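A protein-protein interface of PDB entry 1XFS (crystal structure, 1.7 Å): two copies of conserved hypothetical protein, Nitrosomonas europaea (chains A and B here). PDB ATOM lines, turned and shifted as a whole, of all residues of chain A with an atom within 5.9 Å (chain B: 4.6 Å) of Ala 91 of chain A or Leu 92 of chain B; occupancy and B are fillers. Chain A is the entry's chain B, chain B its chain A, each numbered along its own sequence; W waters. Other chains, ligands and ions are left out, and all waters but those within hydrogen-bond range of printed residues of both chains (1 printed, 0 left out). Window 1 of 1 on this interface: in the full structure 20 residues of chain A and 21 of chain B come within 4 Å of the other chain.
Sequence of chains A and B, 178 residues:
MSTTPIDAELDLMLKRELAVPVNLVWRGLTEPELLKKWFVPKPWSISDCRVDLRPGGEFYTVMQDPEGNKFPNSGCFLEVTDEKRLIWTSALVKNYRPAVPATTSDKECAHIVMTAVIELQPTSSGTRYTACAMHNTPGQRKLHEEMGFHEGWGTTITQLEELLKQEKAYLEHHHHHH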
ATOM      1  N   LEU A  78      -6.524  13.375  -3.067  1.00  0.00           N
ATOM      2  CA  LEU A  78      -6.190  12.713  -4.324  1.00  0.00           C
ATOM      3  C   LEU A  78      -6.565  11.239  -4.317  1.00  0.00           C
ATOM      4  O   LEU A  78      -6.921  10.672  -5.361  1.00  0.00           O
ATOM      5  CB  LEU A  78      -4.695  12.858  -4.594  1.00  0.00           C
ATOM      6  CG  LEU A  78      -4.224  14.314  -4.674  1.00  0.00           C
ATOM      7  CD1 LEU A  78      -2.713  14.347  -4.851  1.00  0.00           C
ATOM      8  CD2 LEU A  78      -4.909  15.029  -5.837  1.00  0.00           C
ATOM      9  N   THR A  89      -2.955  16.898  -1.157  1.00  0.00           N
ATOM     10  CA  THR A  89      -1.878  17.775  -1.571  1.00  0.00           C
ATOM     11  C   THR A  89      -2.248  19.235  -1.383  1.00  0.00           C
ATOM     12  O   THR A  89      -3.428  19.595  -1.385  1.00  0.00           O
ATOM     13  CB  THR A  89      -1.551  17.573  -3.067  1.00  0.00           C
ATOM     14  OG1 THR A  89      -0.419  18.378  -3.431  1.00  0.00           O
ATOM     15  CG2 THR A  89      -2.752  17.960  -3.925  1.00  0.00           C
ATOM     16  N   SER A  90      -1.231  20.074  -1.213  1.00  0.00           N
ATOM     17  CA  SER A  90      -1.468  21.504  -1.095  1.00  0.00           C
ATOM     18  C   SER A  90      -1.067  22.183  -2.416  1.00  0.00           C
ATOM     19  O   SER A  90      -1.129  23.410  -2.535  1.00  0.00           O
ATOM     20  CB  SER A  90      -0.702  22.103   0.096  1.00  0.00           C
ATOM     21  OG  SER A  90       0.692  21.935  -0.015  1.00  0.00           O
ATOM     22  N   ALA A  91      -0.669  21.383  -3.411  1.00  0.00           N
ATOM     23  CA  ALA A  91      -0.288  21.919  -4.721  1.00  0.00           C
ATOM     24  C   ALA A  91      -1.537  22.126  -5.573  1.00  0.00           C
ATOM     25  O   ALA A  91      -1.482  22.745  -6.639  1.00  0.00           O
ATOM     26  CB  ALA A  91       0.694  20.974  -5.436  1.00  0.00           C
ATOM     27  N   LEU A  92      -2.653  21.571  -5.098  1.00  0.00           N
ATOM     28  CA  LEU A  92      -3.947  21.703  -5.757  1.00  0.00           C
ATOM     29  C   LEU A  92      -4.974  22.031  -4.680  1.00  0.00           C
ATOM     30  O   LEU A  92      -4.773  21.743  -3.495  1.00  0.00           O
ATOM     31  CB  LEU A  92      -4.390  20.396  -6.418  1.00  0.00           C
ATOM     32  CG  LEU A  92      -3.529  19.719  -7.479  1.00  0.00           C
ATOM     33  CD1 LEU A  92      -4.229  18.439  -7.935  1.00  0.00           C
ATOM     34  CD2 LEU A  92      -3.317  20.655  -8.665  1.00  0.00           C
ATOM     35  N   VAL A  93      -6.067  22.642  -5.102  1.00  0.00           N
ATOM     36  CA  VAL A  93      -7.149  22.958  -4.191  1.00  0.00           C
ATOM     37  C   VAL A  93      -8.397  22.257  -4.716  1.00  0.00           C
ATOM     38  O   VAL A  93      -8.310  21.396  -5.601  1.00  0.00           O
ATOM     39  CB  VAL A  93      -7.373  24.492  -4.068  1.00  0.00           C
ATOM     40  CG1 VAL A  93      -6.173  25.139  -3.380  1.00  0.00           C
ATOM     41  CG2 VAL A  93      -7.596  25.101  -5.443  1.00  0.00           C
ATOM     42  N   ARG A  97      -7.959  22.044  -8.854  1.00  0.00           N
ATOM     43  CA  ARG A  97      -7.479  23.303  -9.403  1.00  0.00           C
ATOM     44  C   ARG A  97      -6.061  23.586  -8.918  1.00  0.00           C
ATOM     45  O   ARG A  97      -5.757  23.380  -7.748  1.00  0.00           O
ATOM     46  CB  ARG A  97      -8.395  24.452  -8.962  1.00  0.00           C
ATOM     47  CG  ARG A  97      -7.945  25.815  -9.469  1.00  0.00           C
ATOM     48  CD  ARG A  97      -8.908  26.906  -9.004  1.00  0.00           C
ATOM     49  NE  ARG A  97     -10.276  26.668  -9.464  1.00  0.00           N
ATOM     50  CZ  ARG A  97     -10.663  26.719 -10.737  1.00  0.00           C
ATOM     51  NH1 ARG A  97     -11.928  26.489 -11.063  1.00  0.00           N
ATOM     52  NH2 ARG A  97      -9.788  27.005 -11.687  1.00  0.00           N
ATOM     53  N   PRO A  98      -5.170  24.046  -9.809  1.00  0.00           N
ATOM     54  CA  PRO A  98      -3.805  24.334  -9.352  1.00  0.00           C
ATOM     55  C   PRO A  98      -3.841  25.396  -8.257  1.00  0.00           C
ATOM     56  O   PRO A  98      -4.619  26.352  -8.334  1.00  0.00           O
ATOM     57  CB  PRO A  98      -3.111  24.840 -10.615  1.00  0.00           C
ATOM     58  CG  PRO A  98      -3.852  24.125 -11.715  1.00  0.00           C
ATOM     59  CD  PRO A  98      -5.287  24.228 -11.266  1.00  0.00           C
ATOM     60  N   ALA A  99      -3.007  25.223  -7.238  1.00  0.00           N
ATOM     61  CA  ALA A  99      -2.959  26.167  -6.125  1.00  0.00           C
ATOM     62  C   ALA A  99      -2.377  27.517  -6.522  1.00  0.00           C
ATOM     63  O   ALA A  99      -1.648  27.633  -7.509  1.00  0.00           O
ATOM     64  CB  ALA A  99      -2.143  25.575  -4.977  1.00  0.00           C
ATOM     65  N   VAL A 113       4.642  23.889  -0.241  1.00  0.00           N
ATOM     66  CA  VAL A 113       3.840  23.009  -1.085  1.00  0.00           C
ATOM     67  C   VAL A 113       4.225  21.557  -0.820  1.00  0.00           C
ATOM     68  O   VAL A 113       5.407  21.222  -0.792  1.00  0.00           O
ATOM     69  CB  VAL A 113       4.085  23.321  -2.575  1.00  0.00           C
ATOM     70  CG1 VAL A 113       3.243  22.413  -3.451  1.00  0.00           C
ATOM     71  CG2 VAL A 113       3.770  24.785  -2.846  1.00  0.00           C
ATOM     72  N   MET A 114       3.238  20.691  -0.627  1.00  0.00           N
ATOM     73  CA  MET A 114       3.548  19.296  -0.372  1.00  0.00           C
ATOM     74  C   MET A 114       2.412  18.355  -0.716  1.00  0.00           C
ATOM     75  O   MET A 114       1.268  18.772  -0.893  1.00  0.00           O
ATOM     76  CB  MET A 114       3.904  19.104   1.108  1.00  0.00           C
ATOM     77  CG  MET A 114       2.815  19.561   2.079  1.00  0.00           C
ATOM     78  SD  MET A 114       3.030  18.775   3.858  1.00  0.00           S
ATOM     79  CE  MET A 114       2.492  16.981   3.414  1.00  0.00           C
ATOM     80  N   THR A 115       2.755  17.082  -0.857  1.00  0.00           N
ATOM     81  CA  THR A 115       1.754  16.057  -1.075  1.00  0.00           C
ATOM     82  C   THR A 115       2.000  15.061   0.034  1.00  0.00           C
ATOM     83  O   THR A 115       3.119  14.565   0.226  1.00  0.00           O
ATOM     84  CB  THR A 115       1.863  15.352  -2.432  1.00  0.00           C
ATOM     85  OG1 THR A 115       1.451  16.253  -3.467  1.00  0.00           O
ATOM     86  CG2 THR A 115       0.950  14.121  -2.460  1.00  0.00           C
ATOM     87  N   SER B  74       5.989  17.344 -18.099  1.00  0.00           N
ATOM     88  CA  SER B  74       5.729  16.263 -17.159  1.00  0.00           C
ATOM     89  C   SER B  74       4.469  16.567 -16.362  1.00  0.00           C
ATOM     90  O   SER B  74       4.357  17.622 -15.736  1.00  0.00           O
ATOM     91  CB  SER B  74       6.922  16.089 -16.216  1.00  0.00           C
ATOM     92  OG  SER B  74       6.710  15.024 -15.309  1.00  0.00           O
ATOM     93  N   GLY B  75       3.521  15.639 -16.400  1.00  0.00           N
ATOM     94  CA  GLY B  75       2.278  15.834 -15.681  1.00  0.00           C
ATOM     95  C   GLY B  75       1.884  14.576 -14.934  1.00  0.00           C
ATOM     96  O   GLY B  75       2.606  13.576 -14.955  1.00  0.00           O
ATOM     97  N   CYS B  76       0.727  14.623 -14.284  1.00  0.00           N
ATOM     98  CA  CYS B  76       0.238  13.496 -13.491  1.00  0.00           C
ATOM     99  C   CYS B  76      -1.258  13.277 -13.720  1.00  0.00           C
ATOM    100  O   CYS B  76      -2.026  14.231 -13.718  1.00  0.00           O
ATOM    101  CB  CYS B  76       0.486  13.803 -12.005  1.00  0.00           C
ATOM    102  SG  CYS B  76       0.092  12.491 -10.846  1.00  0.00           S
ATOM    103  N   LEU B  78      -4.972  12.348 -12.647  1.00  0.00           N
ATOM    104  CA  LEU B  78      -5.696  12.449 -11.387  1.00  0.00           C
ATOM    105  C   LEU B  78      -6.950  11.590 -11.367  1.00  0.00           C
ATOM    106  O   LEU B  78      -7.359  11.095 -10.318  1.00  0.00           O
ATOM    107  CB  LEU B  78      -6.072  13.901 -11.122  1.00  0.00           C
ATOM    108  CG  LEU B  78      -4.900  14.874 -11.088  1.00  0.00           C
ATOM    109  CD1 LEU B  78      -5.430  16.295 -10.898  1.00  0.00           C
ATOM    110  CD2 LEU B  78      -3.947  14.512  -9.940  1.00  0.00           C
ATOM    111  N   THR B  89      -2.840  16.876 -14.581  1.00  0.00           N
ATOM    112  CA  THR B  89      -2.390  18.185 -14.152  1.00  0.00           C
ATOM    113  C   THR B  89      -0.892  18.356 -14.347  1.00  0.00           C
ATOM    114  O   THR B  89      -0.145  17.379 -14.332  1.00  0.00           O
ATOM    115  CB  THR B  89      -2.714  18.420 -12.651  1.00  0.00           C
ATOM    116  OG1 THR B  89      -2.337  19.754 -12.285  1.00  0.00           O
ATOM    117  CG2 THR B  89      -1.961  17.425 -11.758  1.00  0.00           C
ATOM    118  N   SER B  90      -0.454  19.594 -14.559  1.00  0.00           N
ATOM    119  CA  SER B  90       0.973  19.852 -14.703  1.00  0.00           C
ATOM    120  C   SER B  90       1.498  20.423 -13.391  1.00  0.00           C
ATOM    121  O   SER B  90       2.675  20.733 -13.272  1.00  0.00           O
ATOM    122  CB  SER B  90       1.251  20.800 -15.884  1.00  0.00           C
ATOM    123  OG  SER B  90       0.626  22.048 -15.728  1.00  0.00           O
ATOM    124  N   ALA B  91       0.614  20.543 -12.401  1.00  0.00           N
ATOM    125  CA  ALA B  91       0.993  21.071 -11.084  1.00  0.00           C
ATOM    126  C   ALA B  91       1.664  19.956 -10.286  1.00  0.00           C
ATOM    127  O   ALA B  91       2.340  20.207  -9.279  1.00  0.00           O
ATOM    128  CB  ALA B  91      -0.235  21.571 -10.336  1.00  0.00           C
ATOM    129  N   LEU B  92       1.466  18.720 -10.740  1.00  0.00           N
ATOM    130  CA  LEU B  92       2.053  17.555 -10.089  1.00  0.00           C
ATOM    131  C   LEU B  92       2.717  16.673 -11.138  1.00  0.00           C
ATOM    132  O   LEU B  92       2.353  16.715 -12.314  1.00  0.00           O
ATOM    133  CB  LEU B  92       0.971  16.731  -9.384  1.00  0.00           C
ATOM    134  CG  LEU B  92       0.093  17.383  -8.314  1.00  0.00           C
ATOM    135  CD1 LEU B  92      -0.903  16.349  -7.786  1.00  0.00           C
ATOM    136  CD2 LEU B  92       0.972  17.894  -7.170  1.00  0.00           C
ATOM    137  N   VAL B  93       3.690  15.880 -10.707  1.00  0.00           N
ATOM    138  CA  VAL B  93       4.371  14.961 -11.606  1.00  0.00           C
ATOM    139  C   VAL B  93       4.115  13.539 -11.098  1.00  0.00           C
ATOM    140  O   VAL B  93       3.207  13.317 -10.291  1.00  0.00           O
ATOM    141  CB  VAL B  93       5.903  15.258 -11.702  1.00  0.00           C
ATOM    142  CG1 VAL B  93       6.123  16.616 -12.372  1.00  0.00           C
ATOM    143  CG2 VAL B  93       6.547  15.235 -10.322  1.00  0.00           C
ATOM    144  N   TYR B  96       2.144  11.889  -7.815  1.00  0.00           N
ATOM    145  CA  TYR B  96       1.543  13.069  -7.178  1.00  0.00           C
ATOM    146  C   TYR B  96       2.532  14.045  -6.545  1.00  0.00           C
ATOM    147  O   TYR B  96       2.158  14.836  -5.677  1.00  0.00           O
ATOM    148  CB  TYR B  96       0.544  12.649  -6.096  1.00  0.00           C
ATOM    149  CG  TYR B  96      -0.592  11.758  -6.547  1.00  0.00           C
ATOM    150  CD1 TYR B  96      -1.516  12.190  -7.497  1.00  0.00           C
ATOM    151  CD2 TYR B  96      -0.793  10.511  -5.951  1.00  0.00           C
ATOM    152  CE1 TYR B  96      -2.622  11.405  -7.836  1.00  0.00           C
ATOM    153  CE2 TYR B  96      -1.895   9.719  -6.281  1.00  0.00           C
ATOM    154  CZ  TYR B  96      -2.806  10.179  -7.225  1.00  0.00           C
ATOM    155  OH  TYR B  96      -3.904   9.417  -7.542  1.00  0.00           O
ATOM    156  N   ARG B  97       3.791  13.985  -6.962  1.00  0.00           N
ATOM    157  CA  ARG B  97       4.807  14.886  -6.421  1.00  0.00           C
ATOM    158  C   ARG B  97       4.599  16.312  -6.921  1.00  0.00           C
ATOM    159  O   ARG B  97       4.318  16.521  -8.098  1.00  0.00           O
ATOM    160  CB  ARG B  97       6.200  14.424  -6.854  1.00  0.00           C
ATOM    161  CG  ARG B  97       7.337  15.301  -6.347  1.00  0.00           C
ATOM    162  CD  ARG B  97       8.684  14.758  -6.806  1.00  0.00           C
ATOM    163  NE  ARG B  97       8.945  13.411  -6.294  1.00  0.00           N
ATOM    164  CZ  ARG B  97       9.118  13.124  -5.005  1.00  0.00           C
ATOM    165  NH1 ARG B  97       9.351  11.874  -4.622  1.00  0.00           N
ATOM    166  NH2 ARG B  97       9.062  14.088  -4.095  1.00  0.00           N
ATOM    167  N   PRO B  98       4.714  17.317  -6.033  1.00  0.00           N
ATOM    168  CA  PRO B  98       4.534  18.696  -6.503  1.00  0.00           C
ATOM    169  C   PRO B  98       5.575  18.974  -7.591  1.00  0.00           C
ATOM    170  O   PRO B  98       6.728  18.555  -7.475  1.00  0.00           O
ATOM    171  CB  PRO B  98       4.791  19.524  -5.247  1.00  0.00           C
ATOM    172  CG  PRO B  98       4.224  18.629  -4.158  1.00  0.00           C
ATOM    173  CD  PRO B  98       4.747  17.261  -4.558  1.00  0.00           C
ATOM    174  N   ALA B  99       5.168  19.669  -8.647  1.00  0.00           N
ATOM    175  CA  ALA B  99       6.070  19.984  -9.748  1.00  0.00           C
ATOM    176  C   ALA B  99       7.115  21.031  -9.362  1.00  0.00           C
ATOM    177  O   ALA B  99       6.909  21.835  -8.449  1.00  0.00           O
ATOM    178  CB  ALA B  99       5.263  20.474 -10.949  1.00  0.00           C
HETATM  179  O   HOH W   1      -6.619  11.736  -7.845  1.00  0.00           O
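O of Tyr 96 of chain B sits at hydrogen-bond distance from OG1 of Thr 115 of chain A (2.7 Å).
O of Ala 91 of chain B lies within hydrogen-bond range of N of Ala 99 of chain B, 2.9 Å away.
OG1 of Thr 89 of chain A lies within hydrogen-bond range of N of Ala 91 of chain A (3.0 Å).
O of Met 114 of chain A lies within hydrogen-bond range of OG1 of Thr 89 of chain A.
The side-chain hydroxyl (OG1) of Thr 115 of chain A sits at hydrogen-bond distance from the side-chain hydroxyl (OG1) of Thr 89 of chain A (2.8 Å).
N of Ser 90 of chain A sits at hydrogen-bond distance from O of Met 114 of chain A.
O of Ala 91 of chain A lies within hydrogen-bond range of N of Ala 99 of chain A, at 3.0 Å.
Among the printed residues, merely in contact across the chains: Ala 91 of chain A with Leu 92 of chain B (3.5 Å), Thr 115 of chain A with Pro 98 of chain B (3.6 Å), Leu 78 of chain A with Tyr 96 of chain B (3.6 Å), Leu 92 of chain A with Ala 91 of chain B (3.6 Å), Val 113 of chain A with Pro 98 of chain B (3.7 Å), Leu 92 of chain A with Leu 78 of chain B (3.8 Å), Leu 92 of chain A with Thr 89 of chain B (3.9 Å), Met 114 of chain A with Pro 98 of chain B (3.9 Å), Leu 92 of chain A with Leu 92 of chain B (3.9 Å) and Leu 78 of chain A with Leu 92 of chain B (3.99 Å).
Ala 91 of chain A touches just one residue of chain B: Leu 92.
Of the printed residues of chain A, Leu 92 of chain B touches Leu 78, Ala 91 and Leu 92.
Of the printed residues of chain A, Tyr 96 of chain B touches Leu 78 (3.6 Å) and Thr 115 (2.7 Å).
Printed residues of chain B within 4 Å of Leu 92 of chain A: Leu 78 (3.8 Å), Thr 89 (3.9 Å), Ala 91 (3.6 Å) and Leu 92 (3.9 Å).
Of the printed residues of chain B, Thr 115 of chain A touches Tyr 96 and Pro 98.
Of the printed residues of chain A, Ala 91 of chain B touches Leu 92.
Pro 98 of chain A touches none of the printed residues of chain B.
Printed residues of chain B that touch a printed residue of chain A: Leu 78, Thr 89, Ala 91, Leu 92, Tyr 96 and Pro 98.
Hydrophobic or aromatic side chains of chain B within 4 Å of the printed part of chain A: Leu 78, Ala 91, Leu 92, Tyr 96 and Pro 98.
Among the printed residues, no Asp or Glu carboxylate lies within 4 Å of a Lys or Arg side-chain nitrogen of the other chain.
Leu 78 of chain A touches Leu 92 of chain B, and with the chains exchanged Leu 92 of chain A touches Leu 78 of chain B.
Ala 91 of chain A touches Leu 92 of chain B, and with the chains exchanged Leu 92 of chain A touches Ala 91 of chain B.
Leu 92 of chain A touches Thr 89 of chain B, but with the chains exchanged Thr 89 of chain A does not touch Leu 92 of chain B (4.02 Å).
Leu 92 of chain A touches its own counterpart, Leu 92 of chain B.
Of the 11 pairs that touch across the chains among the printed residues, 5 have their exchanged pair printed and touching as well.
Water W1 lies within hydrogen-bond range of O of Leu 78 of chain B (2.7 Å) and O of Leu 78 of chain A (2.7 Å).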
